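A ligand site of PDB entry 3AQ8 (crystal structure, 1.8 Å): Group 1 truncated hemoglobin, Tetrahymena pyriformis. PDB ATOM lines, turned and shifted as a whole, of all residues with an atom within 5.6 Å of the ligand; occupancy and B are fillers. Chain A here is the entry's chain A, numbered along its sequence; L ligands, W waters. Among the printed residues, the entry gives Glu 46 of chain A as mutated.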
ATOM      1  N   TYR A  25       5.835  14.949 -29.091  1.00  0.00           N
ATOM      2  CA  TYR A  25       6.688  15.886 -29.862  1.00  0.00           C
ATOM      3  C   TYR A  25       6.093  17.272 -29.968  1.00  0.00           C
ATOM      4  O   TYR A  25       6.840  18.238 -29.921  1.00  0.00           O
ATOM      5  CB  TYR A  25       7.017  15.358 -31.289  1.00  0.00           C
ATOM      6  CG  TYR A  25       8.152  14.315 -31.127  1.00  0.00           C
ATOM      7  CD1 TYR A  25       7.912  12.976 -31.350  1.00  0.00           C
ATOM      8  CD2 TYR A  25       9.408  14.727 -30.647  1.00  0.00           C
ATOM      9  CE1 TYR A  25       8.956  11.953 -31.106  1.00  0.00           C
ATOM     10  CE2 TYR A  25      10.447  13.770 -30.389  1.00  0.00           C
ATOM     11  CZ  TYR A  25      10.206  12.405 -30.686  1.00  0.00           C
ATOM     12  OH  TYR A  25      11.168  11.448 -30.402  1.00  0.00           O
ATOM     13  N   VAL A  34      14.266  22.242 -24.517  1.00  0.00           N
ATOM     14  CA  VAL A  34      14.759  21.197 -25.384  1.00  0.00           C
ATOM     15  C   VAL A  34      14.417  21.301 -26.900  1.00  0.00           C
ATOM     16  O   VAL A  34      14.961  20.492 -27.686  1.00  0.00           O
ATOM     17  CB  VAL A  34      14.251  19.813 -24.911  1.00  0.00           C
ATOM     18  CG1 VAL A  34      15.017  19.414 -23.566  1.00  0.00           C
ATOM     19  CG2 VAL A  34      12.746  19.804 -24.677  1.00  0.00           C
ATOM     20  N   PHE A  37      17.130  21.194 -29.802  1.00  0.00           N
ATOM     21  CA  PHE A  37      17.887  19.951 -30.117  1.00  0.00           C
ATOM     22  C   PHE A  37      17.390  19.238 -31.389  1.00  0.00           C
ATOM     23  O   PHE A  37      18.143  18.519 -32.067  1.00  0.00           O
ATOM     24  CB  PHE A  37      17.901  18.975 -28.972  1.00  0.00           C
ATOM     25  CG  PHE A  37      18.754  19.443 -27.837  1.00  0.00           C
ATOM     26  CD1 PHE A  37      18.188  20.076 -26.738  1.00  0.00           C
ATOM     27  CD2 PHE A  37      20.129  19.291 -27.881  1.00  0.00           C
ATOM     28  CE1 PHE A  37      19.009  20.585 -25.680  1.00  0.00           C
ATOM     29  CE2 PHE A  37      20.958  19.799 -26.835  1.00  0.00           C
ATOM     30  CZ  PHE A  37      20.385  20.445 -25.759  1.00  0.00           C
ATOM     31  N   PHE A  38      16.090  19.421 -31.639  1.00  0.00           N
ATOM     32  CA  PHE A  38      15.414  18.885 -32.829  1.00  0.00           C
ATOM     33  C   PHE A  38      15.399  19.734 -34.070  1.00  0.00           C
ATOM     34  O   PHE A  38      14.746  19.345 -35.050  1.00  0.00           O
ATOM     35  CB  PHE A  38      13.978  18.544 -32.357  1.00  0.00           C
ATOM     36  CG  PHE A  38      13.989  17.515 -31.266  1.00  0.00           C
ATOM     37  CD1 PHE A  38      13.965  17.898 -29.930  1.00  0.00           C
ATOM     38  CD2 PHE A  38      14.100  16.196 -31.603  1.00  0.00           C
ATOM     39  CE1 PHE A  38      14.074  16.936 -28.876  1.00  0.00           C
ATOM     40  CE2 PHE A  38      14.208  15.182 -30.587  1.00  0.00           C
ATOM     41  CZ  PHE A  38      14.200  15.552 -29.221  1.00  0.00           C
ATOM     42  N   ASN A  40      17.285  20.112 -36.704  1.00  0.00           N
ATOM     43  CA  ASN A  40      17.646  19.469 -37.985  1.00  0.00           C
ATOM     44  C   ASN A  40      17.143  18.012 -38.069  1.00  0.00           C
ATOM     45  O   ASN A  40      17.508  17.266 -38.979  1.00  0.00           O
ATOM     46  CB  ASN A  40      19.164  19.533 -38.234  1.00  0.00           C
ATOM     47  CG  ASN A  40      19.652  20.942 -38.367  1.00  0.00           C
ATOM     48  OD1 ASN A  40      19.102  21.718 -39.125  1.00  0.00           O
ATOM     49  ND2 ASN A  40      20.696  21.297 -37.620  1.00  0.00           N
ATOM     50  N   THR A  41      16.204  17.671 -37.205  1.00  0.00           N
ATOM     51  CA  THR A  41      15.701  16.253 -37.124  1.00  0.00           C
ATOM     52  C   THR A  41      14.612  15.941 -38.126  1.00  0.00           C
ATOM     53  O   THR A  41      13.712  16.776 -38.347  1.00  0.00           O
ATOM     54  CB  THR A  41      15.162  15.959 -35.717  1.00  0.00           C
ATOM     55  OG1 THR A  41      16.236  16.123 -34.809  1.00  0.00           O
ATOM     56  CG2 THR A  41      14.648  14.475 -35.567  1.00  0.00           C
ATOM     57  N   ASP A  42      14.704  14.779 -38.790  1.00  0.00           N
ATOM     58  CA  ASP A  42      13.656  14.341 -39.717  1.00  0.00           C
ATOM     59  C   ASP A  42      12.553  13.851 -38.739  1.00  0.00           C
ATOM     60  O   ASP A  42      12.712  12.758 -38.096  1.00  0.00           O
ATOM     61  CB  ASP A  42      14.263  13.261 -40.650  1.00  0.00           C
ATOM     62  CG  ASP A  42      13.238  12.449 -41.397  1.00  0.00           C
ATOM     63  OD1 ASP A  42      11.968  12.506 -41.154  1.00  0.00           O
ATOM     64  OD2 ASP A  42      13.724  11.741 -42.343  1.00  0.00           O
ATOM     65  N   HIS A  45      10.911  10.278 -39.418  1.00  0.00           N
ATOM     66  CA  HIS A  45      11.834   9.255 -38.914  1.00  0.00           C
ATOM     67  C   HIS A  45      11.817   9.156 -37.453  1.00  0.00           C
ATOM     68  O   HIS A  45      11.701   8.026 -36.849  1.00  0.00           O
ATOM     69  CB  HIS A  45      13.295   9.497 -39.340  1.00  0.00           C
ATOM     70  CG  HIS A  45      14.205   8.342 -39.006  1.00  0.00           C
ATOM     71  ND1 HIS A  45      15.129   8.391 -37.986  1.00  0.00           N
ATOM     72  CD2 HIS A  45      14.257   7.087 -39.524  1.00  0.00           C
ATOM     73  CE1 HIS A  45      15.766   7.227 -37.913  1.00  0.00           C
ATOM     74  NE2 HIS A  45      15.252   6.418 -38.837  1.00  0.00           N
ATOM     75  N   GLU A  46      12.026  10.279 -36.775  1.00  0.00           N
ATOM     76  CA  GLU A  46      12.122  10.281 -35.372  1.00  0.00           C
ATOM     77  C   GLU A  46      10.814   9.790 -34.647  1.00  0.00           C
ATOM     78  O   GLU A  46      10.875   9.130 -33.611  1.00  0.00           O
ATOM     79  CB  GLU A  46      12.416  11.712 -34.989  1.00  0.00           C
ATOM     80  CG  GLU A  46      12.383  11.997 -33.536  1.00  0.00           C
ATOM     81  CD  GLU A  46      13.475  11.307 -32.741  1.00  0.00           C
ATOM     82  OE1 GLU A  46      14.538  10.925 -33.308  1.00  0.00           O
ATOM     83  OE2 GLU A  46      13.267  11.165 -31.502  1.00  0.00           O
ATOM     84  N   GLN A  49      10.886   5.999 -34.887  1.00  0.00           N
ATOM     85  CA  GLN A  49      11.858   5.361 -33.998  1.00  0.00           C
ATOM     86  C   GLN A  49      11.387   5.424 -32.582  1.00  0.00           C
ATOM     87  O   GLN A  49      11.528   4.443 -31.871  1.00  0.00           O
ATOM     88  CB  GLN A  49      13.252   6.066 -34.058  1.00  0.00           C
ATOM     89  CG  GLN A  49      13.901   5.750 -35.429  1.00  0.00           C
ATOM     90  CD  GLN A  49      13.923   4.242 -35.715  1.00  0.00           C
ATOM     91  OE1 GLN A  49      14.272   3.474 -34.869  1.00  0.00           O
ATOM     92  NE2 GLN A  49      13.559   3.832 -36.862  1.00  0.00           N
ATOM     93  N   GLN A  50      10.847   6.584 -32.167  1.00  0.00           N
ATOM     94  CA  GLN A  50      10.480   6.772 -30.775  1.00  0.00           C
ATOM     95  C   GLN A  50       9.232   5.919 -30.509  1.00  0.00           C
ATOM     96  O   GLN A  50       9.100   5.341 -29.430  1.00  0.00           O
ATOM     97  CB  GLN A  50      10.094   8.265 -30.520  1.00  0.00           C
ATOM     98  CG  GLN A  50       9.746   8.494 -29.027  1.00  0.00           C
ATOM     99  CD  GLN A  50      11.052   8.372 -28.179  1.00  0.00           C
ATOM    100  OE1 GLN A  50      11.280   7.331 -27.530  1.00  0.00           O
ATOM    101  NE2 GLN A  50      11.960   9.333 -28.323  1.00  0.00           N
ATOM    102  N   PHE A  53      10.585   2.540 -30.033  1.00  0.00           N
ATOM    103  CA  PHE A  53      11.360   2.439 -28.794  1.00  0.00           C
ATOM    104  C   PHE A  53      10.481   2.399 -27.512  1.00  0.00           C
ATOM    105  O   PHE A  53      10.631   1.505 -26.662  1.00  0.00           O
ATOM    106  CB  PHE A  53      12.324   3.667 -28.697  1.00  0.00           C
ATOM    107  CG  PHE A  53      13.291   3.532 -27.516  1.00  0.00           C
ATOM    108  CD1 PHE A  53      14.236   2.486 -27.521  1.00  0.00           C
ATOM    109  CD2 PHE A  53      13.188   4.347 -26.418  1.00  0.00           C
ATOM    110  CE1 PHE A  53      15.177   2.313 -26.522  1.00  0.00           C
ATOM    111  CE2 PHE A  53      14.103   4.159 -25.342  1.00  0.00           C
ATOM    112  CZ  PHE A  53      15.136   3.129 -25.426  1.00  0.00           C
ATOM    113  N   LEU A  54       9.505   3.312 -27.394  1.00  0.00           N
ATOM    114  CA  LEU A  54       8.635   3.283 -26.252  1.00  0.00           C
ATOM    115  C   LEU A  54       7.776   2.057 -26.290  1.00  0.00           C
ATOM    116  O   LEU A  54       7.454   1.527 -25.265  1.00  0.00           O
ATOM    117  CB  LEU A  54       7.755   4.545 -26.113  1.00  0.00           C
ATOM    118  CG  LEU A  54       8.677   5.826 -25.931  1.00  0.00           C
ATOM    119  CD1 LEU A  54       7.721   7.077 -25.950  1.00  0.00           C
ATOM    120  CD2 LEU A  54       9.602   5.790 -24.697  1.00  0.00           C
ATOM    121  N   LEU A  57       9.965  -0.606 -24.931  1.00  0.00           N
ATOM    122  CA  LEU A  57      10.419  -0.413 -23.514  1.00  0.00           C
ATOM    123  C   LEU A  57       9.267  -0.713 -22.523  1.00  0.00           C
ATOM    124  O   LEU A  57       9.507  -1.228 -21.423  1.00  0.00           O
ATOM    125  CB  LEU A  57      10.855   1.071 -23.325  1.00  0.00           C
ATOM    126  CG  LEU A  57      11.972   1.348 -22.385  1.00  0.00           C
ATOM    127  CD1 LEU A  57      13.341   0.504 -22.680  1.00  0.00           C
ATOM    128  CD2 LEU A  57      12.301   2.850 -22.599  1.00  0.00           C
ATOM    129  N   TYR A  64      12.043  -2.469 -32.293  1.00  0.00           N
ATOM    130  CA  TYR A  64      12.982  -1.327 -32.252  1.00  0.00           C
ATOM    131  C   TYR A  64      14.300  -1.727 -32.880  1.00  0.00           C
ATOM    132  O   TYR A  64      14.997  -2.641 -32.392  1.00  0.00           O
ATOM    133  CB  TYR A  64      13.182  -0.855 -30.797  1.00  0.00           C
ATOM    134  CG  TYR A  64      14.117   0.344 -30.748  1.00  0.00           C
ATOM    135  CD1 TYR A  64      13.741   1.571 -31.362  1.00  0.00           C
ATOM    136  CD2 TYR A  64      15.373   0.236 -30.188  1.00  0.00           C
ATOM    137  CE1 TYR A  64      14.591   2.660 -31.373  1.00  0.00           C
ATOM    138  CE2 TYR A  64      16.252   1.316 -30.171  1.00  0.00           C
ATOM    139  CZ  TYR A  64      15.843   2.558 -30.825  1.00  0.00           C
ATOM    140  OH  TYR A  64      16.723   3.589 -30.792  1.00  0.00           O
ATOM    141  N   GLY A  66      16.540   0.786 -33.778  1.00  0.00           N
ATOM    142  CA  GLY A  66      17.411   1.978 -33.703  1.00  0.00           C
ATOM    143  C   GLY A  66      18.644   1.951 -32.812  1.00  0.00           C
ATOM    144  O   GLY A  66      19.067   0.903 -32.333  1.00  0.00           O
ATOM    145  N   LYS A  67      19.232   3.135 -32.564  1.00  0.00           N
ATOM    146  CA  LYS A  67      20.475   3.182 -31.921  1.00  0.00           C
ATOM    147  C   LYS A  67      20.230   2.977 -30.410  1.00  0.00           C
ATOM    148  O   LYS A  67      19.143   3.201 -29.907  1.00  0.00           O
ATOM    149  CB  LYS A  67      21.052   4.582 -32.080  1.00  0.00           C
ATOM    150  CG  LYS A  67      21.469   4.886 -33.592  1.00  0.00           C
ATOM    151  CD  LYS A  67      21.969   6.387 -33.720  1.00  0.00           C
ATOM    152  CE  LYS A  67      22.273   6.750 -35.237  1.00  0.00           C
ATOM    153  NZ  LYS A  67      23.496   7.631 -35.226  1.00  0.00           N
ATOM    154  N   MET A  69      20.952   4.160 -26.334  1.00  0.00           N
ATOM    155  CA  MET A  69      20.685   5.503 -25.831  1.00  0.00           C
ATOM    156  C   MET A  69      21.947   6.328 -25.754  1.00  0.00           C
ATOM    157  O   MET A  69      21.874   7.539 -25.719  1.00  0.00           O
ATOM    158  CB  MET A  69      19.923   5.456 -24.507  1.00  0.00           C
ATOM    159  CG  MET A  69      18.445   4.975 -24.690  1.00  0.00           C
ATOM    160  SD  MET A  69      17.445   6.081 -25.764  1.00  0.00           S
ATOM    161  CE  MET A  69      17.546   5.322 -27.404  1.00  0.00           C
ATOM    162  N   ALA A  72      22.533   7.242 -29.622  1.00  0.00           N
ATOM    163  CA  ALA A  72      21.496   8.188 -30.047  1.00  0.00           C
ATOM    164  C   ALA A  72      21.855   9.650 -29.652  1.00  0.00           C
ATOM    165  O   ALA A  72      21.558  10.555 -30.404  1.00  0.00           O
ATOM    166  CB  ALA A  72      20.196   7.857 -29.489  1.00  0.00           C
ATOM    167  N   HIS A  73      22.509   9.857 -28.521  1.00  0.00           N
ATOM    168  CA  HIS A  73      22.672  11.224 -27.978  1.00  0.00           C
ATOM    169  C   HIS A  73      24.150  11.556 -27.895  1.00  0.00           C
ATOM    170  O   HIS A  73      24.549  12.471 -27.119  1.00  0.00           O
ATOM    171  CB  HIS A  73      21.951  11.301 -26.565  1.00  0.00           C
ATOM    172  CG  HIS A  73      20.500  10.908 -26.674  1.00  0.00           C
ATOM    173  ND1 HIS A  73      20.059   9.631 -26.442  1.00  0.00           N
ATOM    174  CD2 HIS A  73      19.442  11.588 -27.174  1.00  0.00           C
ATOM    175  CE1 HIS A  73      18.760   9.568 -26.636  1.00  0.00           C
ATOM    176  NE2 HIS A  73      18.358  10.734 -27.141  1.00  0.00           N
ATOM    177  N   MET A  76      25.972  15.260 -27.794  1.00  0.00           N
ATOM    178  CA  MET A  76      25.004  16.298 -27.388  1.00  0.00           C
ATOM    179  C   MET A  76      25.350  16.870 -25.968  1.00  0.00           C
ATOM    180  O   MET A  76      24.970  17.974 -25.671  1.00  0.00           O
ATOM    181  CB  MET A  76      23.567  15.792 -27.380  1.00  0.00           C
ATOM    182  CG  MET A  76      23.044  15.287 -28.856  1.00  0.00           C
ATOM    183  SD  MET A  76      21.435  14.732 -28.624  1.00  0.00           S
ATOM    184  CE  MET A  76      21.010  14.107 -30.293  1.00  0.00           C
ATOM    185  N   LEU A  78      24.189  16.075 -23.150  1.00  0.00           N
ATOM    186  CA  LEU A  78      22.934  16.393 -22.513  1.00  0.00           C
ATOM    187  C   LEU A  78      23.094  16.511 -20.981  1.00  0.00           C
ATOM    188  O   LEU A  78      23.925  15.828 -20.391  1.00  0.00           O
ATOM    189  CB  LEU A  78      21.905  15.267 -22.742  1.00  0.00           C
ATOM    190  CG  LEU A  78      21.000  15.467 -23.941  1.00  0.00           C
ATOM    191  CD1 LEU A  78      21.196  16.425 -24.896  1.00  0.00           C
ATOM    192  CD2 LEU A  78      20.478  14.006 -24.418  1.00  0.00           C
ATOM    193  N   GLN A  79      22.294  17.383 -20.421  1.00  0.00           N
ATOM    194  CA  GLN A  79      22.357  17.696 -18.967  1.00  0.00           C
ATOM    195  C   GLN A  79      21.032  17.268 -18.286  1.00  0.00           C
ATOM    196  O   GLN A  79      19.982  17.164 -18.898  1.00  0.00           O
ATOM    197  CB  GLN A  79      22.490  19.204 -18.809  1.00  0.00           C
ATOM    198  CG  GLN A  79      23.698  19.809 -19.630  1.00  0.00           C
ATOM    199  CD  GLN A  79      24.958  19.422 -18.983  1.00  0.00           C
ATOM    200  OE1 GLN A  79      25.113  19.543 -17.735  1.00  0.00           O
ATOM    201  NE2 GLN A  79      25.869  18.867 -19.765  1.00  0.00           N
ATOM    202  N   HIS A  82      17.723  18.683 -19.179  1.00  0.00           N
ATOM    203  CA  HIS A  82      17.120  18.276 -20.472  1.00  0.00           C
ATOM    204  C   HIS A  82      16.333  16.983 -20.260  1.00  0.00           C
ATOM    205  O   HIS A  82      15.199  16.857 -20.763  1.00  0.00           O
ATOM    206  CB  HIS A  82      18.210  18.002 -21.511  1.00  0.00           C
ATOM    207  CG  HIS A  82      19.094  19.212 -21.785  1.00  0.00           C
ATOM    208  ND1 HIS A  82      18.599  20.442 -22.180  1.00  0.00           N
ATOM    209  CD2 HIS A  82      20.454  19.335 -21.771  1.00  0.00           C
ATOM    210  CE1 HIS A  82      19.628  21.290 -22.368  1.00  0.00           C
ATOM    211  NE2 HIS A  82      20.744  20.644 -22.156  1.00  0.00           N
ATOM    212  N   PHE A  83      16.923  16.052 -19.517  1.00  0.00           N
ATOM    213  CA  PHE A  83      16.193  14.768 -19.319  1.00  0.00           C
ATOM    214  C   PHE A  83      14.897  15.003 -18.478  1.00  0.00           C
ATOM    215  O   PHE A  83      13.851  14.472 -18.867  1.00  0.00           O
ATOM    216  CB  PHE A  83      17.159  13.746 -18.626  1.00  0.00           C
ATOM    217  CG  PHE A  83      16.560  12.338 -18.523  1.00  0.00           C
ATOM    218  CD1 PHE A  83      16.889  11.391 -19.500  1.00  0.00           C
ATOM    219  CD2 PHE A  83      15.685  12.004 -17.483  1.00  0.00           C
ATOM    220  CE1 PHE A  83      16.357  10.093 -19.477  1.00  0.00           C
ATOM    221  CE2 PHE A  83      15.177  10.714 -17.404  1.00  0.00           C
ATOM    222  CZ  PHE A  83      15.495   9.752 -18.420  1.00  0.00           C
ATOM    223  N   ILE A  86      12.213  16.201 -20.864  1.00  0.00           N
ATOM    224  CA  ILE A  86      11.609  15.127 -21.704  1.00  0.00           C
ATOM    225  C   ILE A  86      10.598  14.322 -20.866  1.00  0.00           C
ATOM    226  O   ILE A  86       9.468  14.080 -21.292  1.00  0.00           O
ATOM    227  CB  ILE A  86      12.702  14.180 -22.294  1.00  0.00           C
ATOM    228  CG1 ILE A  86      13.595  14.938 -23.246  1.00  0.00           C
ATOM    229  CG2 ILE A  86      12.066  12.861 -23.007  1.00  0.00           C
ATOM    230  CD1 ILE A  86      12.898  15.648 -24.422  1.00  0.00           C
ATOM    231  N   ILE A  87      10.955  13.941 -19.645  1.00  0.00           N
ATOM    232  CA  ILE A  87      10.005  13.137 -18.809  1.00  0.00           C
ATOM    233  C   ILE A  87       8.773  13.956 -18.507  1.00  0.00           C
ATOM    234  O   ILE A  87       7.648  13.425 -18.573  1.00  0.00           O
ATOM    235  CB  ILE A  87      10.647  12.757 -17.438  1.00  0.00           C
ATOM    236  CG1 ILE A  87      11.859  11.873 -17.678  1.00  0.00           C
ATOM    237  CG2 ILE A  87       9.590  12.086 -16.450  1.00  0.00           C
ATOM    238  CD1 ILE A  87      11.415  10.410 -18.290  1.00  0.00           C
ATOM    239  N   ILE A 111      11.409   4.353 -17.959  1.00  0.00           N
ATOM    240  CA  ILE A 111      12.233   5.274 -18.797  1.00  0.00           C
ATOM    241  C   ILE A 111      13.361   5.899 -18.054  1.00  0.00           C
ATOM    242  O   ILE A 111      14.444   6.129 -18.597  1.00  0.00           O
ATOM    243  CB  ILE A 111      11.298   6.378 -19.387  1.00  0.00           C
ATOM    244  CG1 ILE A 111      10.291   5.628 -20.249  1.00  0.00           C
ATOM    245  CG2 ILE A 111      12.106   7.461 -20.154  1.00  0.00           C
ATOM    246  CD1 ILE A 111       9.016   6.392 -20.596  1.00  0.00           C
ATOM    247  N   THR A 114      17.128   5.013 -18.249  1.00  0.00           N
ATOM    248  CA  THR A 114      17.955   5.426 -19.448  1.00  0.00           C
ATOM    249  C   THR A 114      18.771   6.665 -19.161  1.00  0.00           C
ATOM    250  O   THR A 114      19.650   7.008 -19.970  1.00  0.00           O
ATOM    251  CB  THR A 114      17.119   5.688 -20.695  1.00  0.00           C
ATOM    252  OG1 THR A 114      16.237   6.824 -20.542  1.00  0.00           O
ATOM    253  CG2 THR A 114      16.272   4.452 -21.080  1.00  0.00           C
ATOM    254  N   MET A 118      22.443   8.378 -21.429  1.00  0.00           N
ATOM    255  CA  MET A 118      22.427   9.476 -22.362  1.00  0.00           C
ATOM    256  C   MET A 118      22.987  10.820 -21.880  1.00  0.00           C
ATOM    257  O   MET A 118      23.276  11.664 -22.727  1.00  0.00           O
ATOM    258  CB  MET A 118      21.025   9.660 -22.932  1.00  0.00           C
ATOM    259  CG  MET A 118      19.976  10.115 -21.890  1.00  0.00           C
ATOM    260  SD  MET A 118      18.438  10.349 -22.725  1.00  0.00           S
ATOM    261  CE  MET A 118      17.910   8.655 -23.076  1.00  0.00           C
ATOM    262  N   LEU A 119      23.105  11.063 -20.568  1.00  0.00           N
ATOM    263  CA  LEU A 119      23.609  12.362 -20.092  1.00  0.00           C
ATOM    264  C   LEU A 119      25.125  12.448 -20.337  1.00  0.00           C
ATOM    265  O   LEU A 119      25.877  11.462 -20.118  1.00  0.00           O
ATOM    266  CB  LEU A 119      23.398  12.602 -18.571  1.00  0.00           C
ATOM    267  CG  LEU A 119      21.885  12.695 -18.211  1.00  0.00           C
ATOM    268  CD1 LEU A 119      21.861  13.131 -16.727  1.00  0.00           C
ATOM    269  CD2 LEU A 119      21.171  13.755 -19.177  1.00  0.00           C
HETATM  270  C1  LIG L   1      17.313  10.476 -30.870  1.00  0.00           C
HETATM  271  C2  LIG L   1      17.195  14.605 -28.206  1.00  0.00           C
HETATM  272  C3  LIG L   1      16.134  12.016 -24.241  1.00  0.00           C
HETATM  273  C4  LIG L   1      14.957   8.389 -27.164  1.00  0.00           C
HETATM  274  C5  LIG L   1      17.354  11.791 -30.510  1.00  0.00           C
HETATM  275  C6  LIG L   1      17.691  12.927 -31.395  1.00  0.00           C
HETATM  276  C7  LIG L   1      17.616  14.051 -30.631  1.00  0.00           C
HETATM  277  C8  LIG L   1      17.304  13.687 -29.246  1.00  0.00           C
HETATM  278  C9  LIG L   1      17.847  15.534 -31.024  1.00  0.00           C
HETATM  279  C10 LIG L   1      17.854  12.802 -32.945  1.00  0.00           C
HETATM  280  C11 LIG L   1      19.199  13.135 -33.535  1.00  0.00           C
HETATM  281  C12 LIG L   1      18.617  13.240 -34.995  1.00  0.00           C
HETATM  282  O1  LIG L   1      18.370  12.099 -35.560  1.00  0.00           O
HETATM  283  O2  LIG L   1      18.175  14.361 -35.478  1.00  0.00           O
HETATM  284  C13 LIG L   1      16.966  14.236 -26.894  1.00  0.00           C
HETATM  285  C14 LIG L   1      17.128  15.160 -25.755  1.00  0.00           C
HETATM  286  C15 LIG L   1      16.867  14.432 -24.633  1.00  0.00           C
HETATM  287  C16 LIG L   1      16.549  13.041 -25.087  1.00  0.00           C
HETATM  288  C17 LIG L   1      17.452  16.667 -25.778  1.00  0.00           C
HETATM  289  C18 LIG L   1      16.892  14.963 -23.163  1.00  0.00           C
HETATM  290  C19 LIG L   1      17.584  14.193 -22.347  1.00  0.00           C
HETATM  291  C20 LIG L   1      15.546  10.855 -24.670  1.00  0.00           C
HETATM  292  C21 LIG L   1      14.776   9.864 -23.864  1.00  0.00           C
HETATM  293  C22 LIG L   1      14.451   8.844 -24.724  1.00  0.00           C
HETATM  294  C23 LIG L   1      14.984   9.180 -26.046  1.00  0.00           C
HETATM  295  C24 LIG L   1      14.419  10.093 -22.377  1.00  0.00           C
HETATM  296  C25 LIG L   1      13.588   7.591 -24.540  1.00  0.00           C
HETATM  297  C26 LIG L   1      13.463   7.172 -23.316  1.00  0.00           C
HETATM  298  C27 LIG L   1      15.504   8.610 -28.386  1.00  0.00           C
HETATM  299  C28 LIG L   1      15.386   7.649 -29.484  1.00  0.00           C
HETATM  300  C29 LIG L   1      16.133   8.308 -30.621  1.00  0.00           C
HETATM  301  C30 LIG L   1      16.594   9.570 -30.100  1.00  0.00           C
HETATM  302  C31 LIG L   1      14.633   6.304 -29.582  1.00  0.00           C
HETATM  303  C32 LIG L   1      16.264   7.717 -32.041  1.00  0.00           C
HETATM  304  C33 LIG L   1      17.558   6.987 -32.213  1.00  0.00           C
HETATM  305  C34 LIG L   1      17.571   6.463 -33.650  1.00  0.00           C
HETATM  306  O3  LIG L   1      18.015   5.314 -33.901  1.00  0.00           O
HETATM  307  O4  LIG L   1      17.223   7.317 -34.583  1.00  0.00           O
HETATM  308  N1  LIG L   1      17.184  12.337 -29.270  1.00  0.00           N
HETATM  309  N2  LIG L   1      16.670  12.931 -26.463  1.00  0.00           N
HETATM  310  N3  LIG L   1      15.645  10.332 -25.874  1.00  0.00           N
HETATM  311  N4  LIG L   1      16.230   9.726 -28.770  1.00  0.00           N
HETATM  312 FE1  LIG L   1      16.452  11.345 -27.574  1.00  0.00          FE
HETATM  313  O   HOH W   1      18.774   9.675 -34.639  1.00  0.00           O
HETATM  314  O   HOH W   2      14.257  11.997 -28.184  1.00  0.00           O
HETATM  315  O   HOH W   3      16.708  13.008 -38.246  1.00  0.00           O
HETATM  316  O   HOH W   4      21.036  10.243 -33.039  1.00  0.00           O
HETATM  317  O   HOH W   5      18.566   4.589 -36.389  1.00  0.00           O
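O2 of the ligand lies within hydrogen-bond range of OG1 of Thr 41.
FE1 of the ligand is bound by NE2 of His 73.
N of Lys 67 is in hydrogen-bond range of O3 of the ligand (2.8 Å).
NE2 of Gln 50 sits at hydrogen-bond distance from OH of Tyr 25 (3.1 Å).
O of Met 69 is in hydrogen-bond range of ND1 of His 73, 2.9 Å away.
The backbone carbonyl oxygen (O) of Lys 67 sits at hydrogen-bond distance from the side-chain hydroxyl (OH) of Tyr 64.
The side-chain hydroxyl of Thr 114 is in hydrogen-bond range of the backbone carbonyl oxygen of Ile 111.
OD1 of Asp 42 lies within hydrogen-bond range of N of His 45, at 3.0 Å.
Phe 37 touches the ligand (O to C9, 3.2 Å).
CZ of Phe 38 touches C2 of the ligand (3.3 Å).
His 45 touches the ligand (CE1 to O4, 3.6 Å).
Glu 46 touches the ligand (OE1 to C1, 3.7 Å).
CG of Gln 49 touches O4 of the ligand, at 3.8 Å.
Gln 50 touches the ligand (NE2 to C4, 3.3 Å).
CE2 of Phe 53 touches C25 of the ligand, at 3.6 Å.
OH of Tyr 64 touches C31 of the ligand, at 3.6 Å.
Gly 66 touches the ligand (CA to O3, 3.4 Å).
Met 69 touches the ligand.
Ala 72 touches the ligand.
Met 76 touches the ligand (CE to C7, 3.4 Å).
Leu 78 touches the ligand.
O of His 82 touches C18 of the ligand, 3.5 Å away.
CA of Phe 83 touches C19 of the ligand (3.4 Å).
Ile 86 touches the ligand.
Ile 111 touches the ligand.
Thr 114 touches the ligand (OG1 to C26, 3.9 Å).
SD of Met 118 touches C3 of the ligand, at 3.2 Å.
Hydrophobic or aromatic side chains that line the ligand: Phe 37, Phe 38, His 45, Phe 53, Met 69, Ala 72, His 73, Met 76, Leu 78, His 82, Phe 83, Ile 86, Ile 111 and Met 118.
Within 4 Å of the ligand: Phe 37, Phe 38, Thr 41, His 45, Glu 46, Gln 49, Gln 50, Phe 53, Tyr 64, Gly 66, Lys 67, Met 69, Ala 72, His 73, Met 76, Leu 78, His 82, Phe 83, Ile 86, Ile 111, Thr 114 and Met 118.
The nearest printed residue that does not touch the ligand is Val 34 (4.3 Å).
Water W3 bridges N of Asp 42 (2.7 Å) and O1 of the ligand (3.3 Å).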
